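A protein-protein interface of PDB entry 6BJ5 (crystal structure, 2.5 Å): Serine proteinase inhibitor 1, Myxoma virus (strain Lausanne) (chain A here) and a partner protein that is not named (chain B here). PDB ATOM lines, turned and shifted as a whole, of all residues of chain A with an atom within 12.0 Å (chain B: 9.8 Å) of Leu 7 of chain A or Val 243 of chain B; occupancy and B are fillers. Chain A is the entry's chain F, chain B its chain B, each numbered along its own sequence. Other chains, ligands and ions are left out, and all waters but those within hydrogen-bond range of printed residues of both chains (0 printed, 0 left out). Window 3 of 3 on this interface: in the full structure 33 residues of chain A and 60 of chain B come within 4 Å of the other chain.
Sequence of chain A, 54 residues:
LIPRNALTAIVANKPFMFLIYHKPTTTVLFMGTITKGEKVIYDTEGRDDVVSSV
The backbone carbonyl oxygen (O) of Gln 245 of chain B is in hydrogen-bond range of the backbone NH (N) of Ile 10 of chain A, at 2.8 Å.
The side-chain hydroxyl (OG1) of Thr 8 of chain A lies within hydrogen-bond range of the side-chain carboxylate (OD1) of Asp 242 of chain B.
The backbone carbonyl oxygen (O) of Thr 8 of chain A lies within hydrogen-bond range of the backbone NH (N) of Gln 245 of chain B (2.9 Å).
The side-chain hydroxyl (OG1) of Thr 188 of chain B lies within hydrogen-bond range of the backbone carbonyl oxygen (O) of Leu 186 of chain B.
N of Arg 240 of chain B is in hydrogen-bond range of O of Thr 188 of chain B, at 2.7 Å.
The backbone carbonyl oxygen (O) of Asp 242 of chain B lies within hydrogen-bond range of the backbone NH (N) of Leu 186 of chain B (3.1 Å).
OG1 of Thr 188 of chain B sits at hydrogen-bond distance from SG of Cys 244 of chain B (3.2 Å).
The backbone carbonyl oxygen of Lys 182 of chain B lies within hydrogen-bond range of the backbone NH of Val 246 of chain B (2.9 Å).
The side-chain amide oxygen of Asn 181 of chain B sits at hydrogen-bond distance from the side-chain amide nitrogen of Gln 245 of chain B, at 3.1 Å.
O of Val 243 of chain B touches CD1 of Leu 7 of chain A, at 3.2 Å.
Thr 8 of chain A touches Val 243 of chain B (CB to O, 3.6 Å).
O of Thr 8 of chain A touches CA of Cys 244 of chain B, 3.3 Å away.
CA of Ala 9 of chain A touches O of Gln 245 of chain B (3.6 Å).
Thr 188 of chain B touches Ile 10 of chain A (CG2 to CD1, 3.99 Å).
CG1 of Ile 10 of chain A touches OG1 of Thr 201 of chain B, at 3.5 Å.
Cys 244 of chain B touches Ile 10 of chain A.
O of Ile 10 of chain A touches CA of Val 246 of chain B, at 3.6 Å.
Printed residues of chain B within 4 Å of Leu 7 of chain A: Val 243 (3.2 Å).
Of chain A, only Leu 7 and Thr 8 come within 4 Å of Val 243 of chain B.
Of chain B, only Asp 242 (2.9 Å), Val 243 (3.6 Å), Cys 244 (3.3 Å) and Gln 245 (2.9 Å) come within 4 Å of Thr 8 of chain A.
No residue of chain A comes within 4 Å of Ile 183 of chain B.
No residue of chain A comes within 4 Å of Thr 185 of chain B.
Asp 242 of chain B touches just one residue of chain A: Thr 8 (2.9 Å).
Cys 244 of chain B touches two residues of chain A.
Printed residues of chain A within 4 Å of Thr 201 of chain B: Ile 10 (3.5 Å).
Of the printed residues of chain A, Thr 188 of chain B touches Ile 10.
Of the printed residues of chain B, Ile 10 of chain A touches Thr 188, Thr 201, Cys 244, Gln 245 and Val 246.
Asp 184 of chain B touches none of the printed residues of chain A.
Arg 240 of chain B touches none of the printed residues of chain A.
Along chain B the printed residues that touch a printed residue of chain A span positions 188 to 246.
Among the printed residues, 11 pairs touch across the chains.
Among the printed residues, no Asp or Glu carboxylate lies within 4 Å of a Lys or Arg side-chain nitrogen of the other chain.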
ATOM      1  N   LEU A   7       2.137  16.645  34.615  1.00  0.00           N
ATOM      2  CA  LEU A   7       2.190  17.066  33.214  1.00  0.00           C
ATOM      3  C   LEU A   7       0.769  17.288  32.672  1.00  0.00           C
ATOM      4  O   LEU A   7      -0.188  16.789  33.267  1.00  0.00           O
ATOM      5  CB  LEU A   7       2.956  16.026  32.403  1.00  0.00           C
ATOM      6  CG  LEU A   7       2.972  16.151  30.898  1.00  0.00           C
ATOM      7  CD1 LEU A   7       3.796  17.373  30.620  1.00  0.00           C
ATOM      8  CD2 LEU A   7       3.636  14.932  30.307  1.00  0.00           C
ATOM      9  N   THR A   8       0.619  18.028  31.563  1.00  0.00           N
ATOM     10  CA  THR A   8      -0.711  18.360  31.037  1.00  0.00           C
ATOM     11  C   THR A   8      -1.396  17.162  30.364  1.00  0.00           C
ATOM     12  O   THR A   8      -0.940  16.673  29.324  1.00  0.00           O
ATOM     13  CB  THR A   8      -0.614  19.522  30.057  1.00  0.00           C
ATOM     14  OG1 THR A   8      -0.031  20.651  30.717  1.00  0.00           O
ATOM     15  CG2 THR A   8      -2.015  19.915  29.579  1.00  0.00           C
ATOM     16  N   ALA A   9      -2.542  16.751  30.902  1.00  0.00           N
ATOM     17  CA  ALA A   9      -3.226  15.539  30.470  1.00  0.00           C
ATOM     18  C   ALA A   9      -4.595  15.895  29.912  1.00  0.00           C
ATOM     19  O   ALA A   9      -5.456  16.391  30.652  1.00  0.00           O
ATOM     20  CB  ALA A   9      -3.386  14.561  31.628  1.00  0.00           C
ATOM     21  N   ILE A  10      -4.806  15.573  28.634  1.00  0.00           N
ATOM     22  CA  ILE A  10      -6.085  15.716  27.943  1.00  0.00           C
ATOM     23  C   ILE A  10      -6.678  14.318  27.786  1.00  0.00           C
ATOM     24  O   ILE A  10      -6.125  13.471  27.072  1.00  0.00           O
ATOM     25  CB  ILE A  10      -5.914  16.409  26.576  1.00  0.00           C
ATOM     26  CG1 ILE A  10      -5.375  17.822  26.748  1.00  0.00           C
ATOM     27  CG2 ILE A  10      -7.220  16.443  25.796  1.00  0.00           C
ATOM     28  CD1 ILE A  10      -3.925  17.935  26.405  1.00  0.00           C
ATOM     29  N   VAL A  11      -7.800  14.061  28.449  1.00  0.00           N
ATOM     30  CA  VAL A  11      -8.420  12.742  28.438  1.00  0.00           C
ATOM     31  C   VAL A  11      -9.848  12.897  27.962  1.00  0.00           C
ATOM     32  O   VAL A  11     -10.710  13.377  28.711  1.00  0.00           O
ATOM     33  CB  VAL A  11      -8.398  12.059  29.809  1.00  0.00           C
ATOM     34  CG1 VAL A  11      -9.037  10.659  29.699  1.00  0.00           C
ATOM     35  CG2 VAL A  11      -6.974  11.990  30.363  1.00  0.00           C
ATOM     36  N   ASN B 181      -3.384   6.770  22.879  1.00  0.00           N
ATOM     37  CA  ASN B 181      -2.612   7.408  23.938  1.00  0.00           C
ATOM     38  C   ASN B 181      -1.246   7.799  23.394  1.00  0.00           C
ATOM     39  O   ASN B 181      -0.547   6.960  22.813  1.00  0.00           O
ATOM     40  CB  ASN B 181      -2.458   6.464  25.135  1.00  0.00           C
ATOM     41  CG  ASN B 181      -1.683   7.086  26.299  1.00  0.00           C
ATOM     42  OD1 ASN B 181      -1.243   8.236  26.250  1.00  0.00           O
ATOM     43  ND2 ASN B 181      -1.510   6.304  27.354  1.00  0.00           N
ATOM     44  N   LYS B 182      -0.877   9.070  23.559  1.00  0.00           N
ATOM     45  CA  LYS B 182       0.445   9.517  23.123  1.00  0.00           C
ATOM     46  C   LYS B 182       0.902  10.732  23.929  1.00  0.00           C
ATOM     47  O   LYS B 182       0.104  11.427  24.581  1.00  0.00           O
ATOM     48  CB  LYS B 182       0.469   9.857  21.626  1.00  0.00           C
ATOM     49  CG  LYS B 182      -0.013  11.303  21.317  1.00  0.00           C
ATOM     50  CD  LYS B 182       0.056  11.585  19.830  1.00  0.00           C
ATOM     51  CE  LYS B 182      -0.848  12.715  19.423  1.00  0.00           C
ATOM     52  NZ  LYS B 182      -0.309  13.348  18.178  1.00  0.00           N
ATOM     53  N   ILE B 183       2.208  10.990  23.854  1.00  0.00           N
ATOM     54  CA  ILE B 183       2.797  12.227  24.354  1.00  0.00           C
ATOM     55  C   ILE B 183       3.210  13.065  23.158  1.00  0.00           C
ATOM     56  O   ILE B 183       3.756  12.542  22.176  1.00  0.00           O
ATOM     57  CB  ILE B 183       3.991  11.975  25.291  1.00  0.00           C
ATOM     58  CG1 ILE B 183       3.495  11.445  26.641  1.00  0.00           C
ATOM     59  CG2 ILE B 183       4.801  13.244  25.462  1.00  0.00           C
ATOM     60  CD1 ILE B 183       4.586  10.843  27.500  1.00  0.00           C
ATOM     61  N   ASP B 184       2.880  14.352  23.213  1.00  0.00           N
ATOM     62  CA  ASP B 184       3.109  15.240  22.085  1.00  0.00           C
ATOM     63  C   ASP B 184       3.037  16.659  22.630  1.00  0.00           C
ATOM     64  O   ASP B 184       2.395  16.908  23.660  1.00  0.00           O
ATOM     65  CB  ASP B 184       2.066  14.982  20.978  1.00  0.00           C
ATOM     66  CG  ASP B 184       2.426  15.606  19.642  1.00  0.00           C
ATOM     67  OD1 ASP B 184       3.372  16.413  19.593  1.00  0.00           O
ATOM     68  OD2 ASP B 184       1.751  15.272  18.638  1.00  0.00           O
ATOM     69  N   THR B 185       3.722  17.578  21.945  1.00  0.00           N
ATOM     70  CA  THR B 185       3.646  19.014  22.222  1.00  0.00           C
ATOM     71  C   THR B 185       2.744  19.701  21.209  1.00  0.00           C
ATOM     72  O   THR B 185       3.000  19.653  19.994  1.00  0.00           O
ATOM     73  CB  THR B 185       5.023  19.684  22.306  1.00  0.00           C
ATOM     74  OG1 THR B 185       5.961  18.835  22.985  1.00  0.00           O
ATOM     75  CG2 THR B 185       4.954  21.100  22.874  1.00  0.00           C
ATOM     76  N   LEU B 186       1.705  20.351  21.745  1.00  0.00           N
ATOM     77  CA  LEU B 186       0.521  20.819  21.051  1.00  0.00           C
ATOM     78  C   LEU B 186       0.016  22.083  21.736  1.00  0.00           C
ATOM     79  O   LEU B 186       0.207  22.260  22.942  1.00  0.00           O
ATOM     80  CB  LEU B 186      -0.590  19.778  21.138  1.00  0.00           C
ATOM     81  CG  LEU B 186      -0.297  18.317  20.841  1.00  0.00           C
ATOM     82  CD1 LEU B 186      -1.478  17.480  21.357  1.00  0.00           C
ATOM     83  CD2 LEU B 186      -0.009  18.080  19.349  1.00  0.00           C
ATOM     84  N   LYS B 187      -0.712  22.910  20.991  1.00  0.00           N
ATOM     85  CA  LYS B 187      -1.361  24.066  21.603  1.00  0.00           C
ATOM     86  C   LYS B 187      -2.568  23.604  22.421  1.00  0.00           C
ATOM     87  O   LYS B 187      -3.319  22.723  21.990  1.00  0.00           O
ATOM     88  CB  LYS B 187      -1.759  25.089  20.523  1.00  0.00           C
ATOM     89  CG  LYS B 187      -0.554  25.635  19.727  1.00  0.00           C
ATOM     90  CD  LYS B 187      -0.913  26.712  18.705  1.00  0.00           C
ATOM     91  CE  LYS B 187       0.106  26.746  17.560  1.00  0.00           C
ATOM     92  NZ  LYS B 187      -0.323  27.627  16.442  1.00  0.00           N
ATOM     93  N   THR B 188      -2.743  24.186  23.615  1.00  0.00           N
ATOM     94  CA  THR B 188      -3.803  23.791  24.539  1.00  0.00           C
ATOM     95  C   THR B 188      -4.116  24.974  25.437  1.00  0.00           C
ATOM     96  O   THR B 188      -3.342  25.931  25.514  1.00  0.00           O
ATOM     97  CB  THR B 188      -3.385  22.616  25.445  1.00  0.00           C
ATOM     98  OG1 THR B 188      -2.516  21.725  24.750  1.00  0.00           O
ATOM     99  CG2 THR B 188      -4.601  21.843  25.947  1.00  0.00           C
ATOM    100  N   THR B 201      -7.590  21.598  22.310  1.00  0.00           N
ATOM    101  CA  THR B 201      -6.268  21.103  21.968  1.00  0.00           C
ATOM    102  C   THR B 201      -6.194  20.913  20.462  1.00  0.00           C
ATOM    103  O   THR B 201      -7.105  20.337  19.866  1.00  0.00           O
ATOM    104  CB  THR B 201      -5.999  19.775  22.701  1.00  0.00           C
ATOM    105  OG1 THR B 201      -6.138  19.969  24.119  1.00  0.00           O
ATOM    106  CG2 THR B 201      -4.613  19.231  22.368  1.00  0.00           C
ATOM    107  N   ARG B 240      -2.027  27.827  24.054  1.00  0.00           N
ATOM    108  CA  ARG B 240      -0.591  28.012  24.204  1.00  0.00           C
ATOM    109  C   ARG B 240       0.093  26.658  24.112  1.00  0.00           C
ATOM    110  O   ARG B 240      -0.426  25.663  24.631  1.00  0.00           O
ATOM    111  CB  ARG B 240      -0.258  28.688  25.546  1.00  0.00           C
ATOM    112  CG  ARG B 240      -1.234  29.780  25.947  1.00  0.00           C
ATOM    113  CD  ARG B 240      -0.569  31.148  25.977  1.00  0.00           C
ATOM    114  NE  ARG B 240       0.101  31.496  24.723  1.00  0.00           N
ATOM    115  CZ  ARG B 240      -0.497  32.067  23.682  1.00  0.00           C
ATOM    116  NH1 ARG B 240      -1.790  32.350  23.730  1.00  0.00           N
ATOM    117  NH2 ARG B 240       0.202  32.351  22.593  1.00  0.00           N
ATOM    118  N   LYS B 241       1.249  26.619  23.451  1.00  0.00           N
ATOM    119  CA  LYS B 241       1.981  25.371  23.341  1.00  0.00           C
ATOM    120  C   LYS B 241       2.358  24.844  24.740  1.00  0.00           C
ATOM    121  O   LYS B 241       2.360  25.581  25.733  1.00  0.00           O
ATOM    122  CB  LYS B 241       3.203  25.560  22.448  1.00  0.00           C
ATOM    123  CG  LYS B 241       3.864  24.249  22.073  1.00  0.00           C
ATOM    124  CD  LYS B 241       5.088  24.387  21.178  1.00  0.00           C
ATOM    125  CE  LYS B 241       4.759  24.236  19.705  1.00  0.00           C
ATOM    126  NZ  LYS B 241       6.007  24.176  18.881  1.00  0.00           N
ATOM    127  N   ASP B 242       2.640  23.538  24.812  1.00  0.00           N
ATOM    128  CA  ASP B 242       2.760  22.779  26.061  1.00  0.00           C
ATOM    129  C   ASP B 242       2.999  21.312  25.694  1.00  0.00           C
ATOM    130  O   ASP B 242       2.580  20.856  24.630  1.00  0.00           O
ATOM    131  CB  ASP B 242       1.477  22.943  26.897  1.00  0.00           C
ATOM    132  CG  ASP B 242       1.524  22.232  28.238  1.00  0.00           C
ATOM    133  OD1 ASP B 242       1.049  22.830  29.219  1.00  0.00           O
ATOM    134  OD2 ASP B 242       1.994  21.080  28.326  1.00  0.00           O
ATOM    135  N   VAL B 243       3.676  20.579  26.580  1.00  0.00           N
ATOM    136  CA  VAL B 243       3.868  19.135  26.418  1.00  0.00           C
ATOM    137  C   VAL B 243       2.628  18.412  26.928  1.00  0.00           C
ATOM    138  O   VAL B 243       2.241  18.564  28.093  1.00  0.00           O
ATOM    139  CB  VAL B 243       5.125  18.668  27.167  1.00  0.00           C
ATOM    140  CG1 VAL B 243       5.209  17.149  27.193  1.00  0.00           C
ATOM    141  CG2 VAL B 243       6.355  19.263  26.533  1.00  0.00           C
ATOM    142  N   CYS B 244       2.013  17.594  26.089  1.00  0.00           N
ATOM    143  CA  CYS B 244       0.756  16.993  26.493  1.00  0.00           C
ATOM    144  C   CYS B 244       0.775  15.485  26.377  1.00  0.00           C
ATOM    145  O   CYS B 244       1.516  14.898  25.574  1.00  0.00           O
ATOM    146  CB  CYS B 244      -0.441  17.479  25.654  1.00  0.00           C
ATOM    147  SG  CYS B 244      -0.794  19.212  25.673  1.00  0.00           S
ATOM    148  N   GLN B 245      -0.084  14.888  27.202  1.00  0.00           N
ATOM    149  CA  GLN B 245      -0.562  13.526  27.045  1.00  0.00           C
ATOM    150  C   GLN B 245      -1.985  13.621  26.504  1.00  0.00           C
ATOM    151  O   GLN B 245      -2.862  14.224  27.141  1.00  0.00           O
ATOM    152  CB  GLN B 245      -0.526  12.744  28.363  1.00  0.00           C
ATOM    153  CG  GLN B 245      -0.669  11.228  28.124  1.00  0.00           C
ATOM    154  CD  GLN B 245      -0.903  10.401  29.384  1.00  0.00           C
ATOM    155  OE1 GLN B 245      -0.990  10.933  30.486  1.00  0.00           O
ATOM    156  NE2 GLN B 245      -1.027   9.085  29.212  1.00  0.00           N
ATOM    157  N   VAL B 246      -2.205  13.038  25.329  1.00  0.00           N
ATOM    158  CA  VAL B 246      -3.515  12.985  24.690  1.00  0.00           C
ATOM    159  C   VAL B 246      -4.021  11.554  24.776  1.00  0.00           C
ATOM    160  O   VAL B 246      -3.360  10.626  24.295  1.00  0.00           O
ATOM    161  CB  VAL B 246      -3.435  13.466  23.235  1.00  0.00           C
ATOM    162  CG1 VAL B 246      -4.780  13.402  22.556  1.00  0.00           C
ATOM    163  CG2 VAL B 246      -2.863  14.857  23.197  1.00  0.00           C
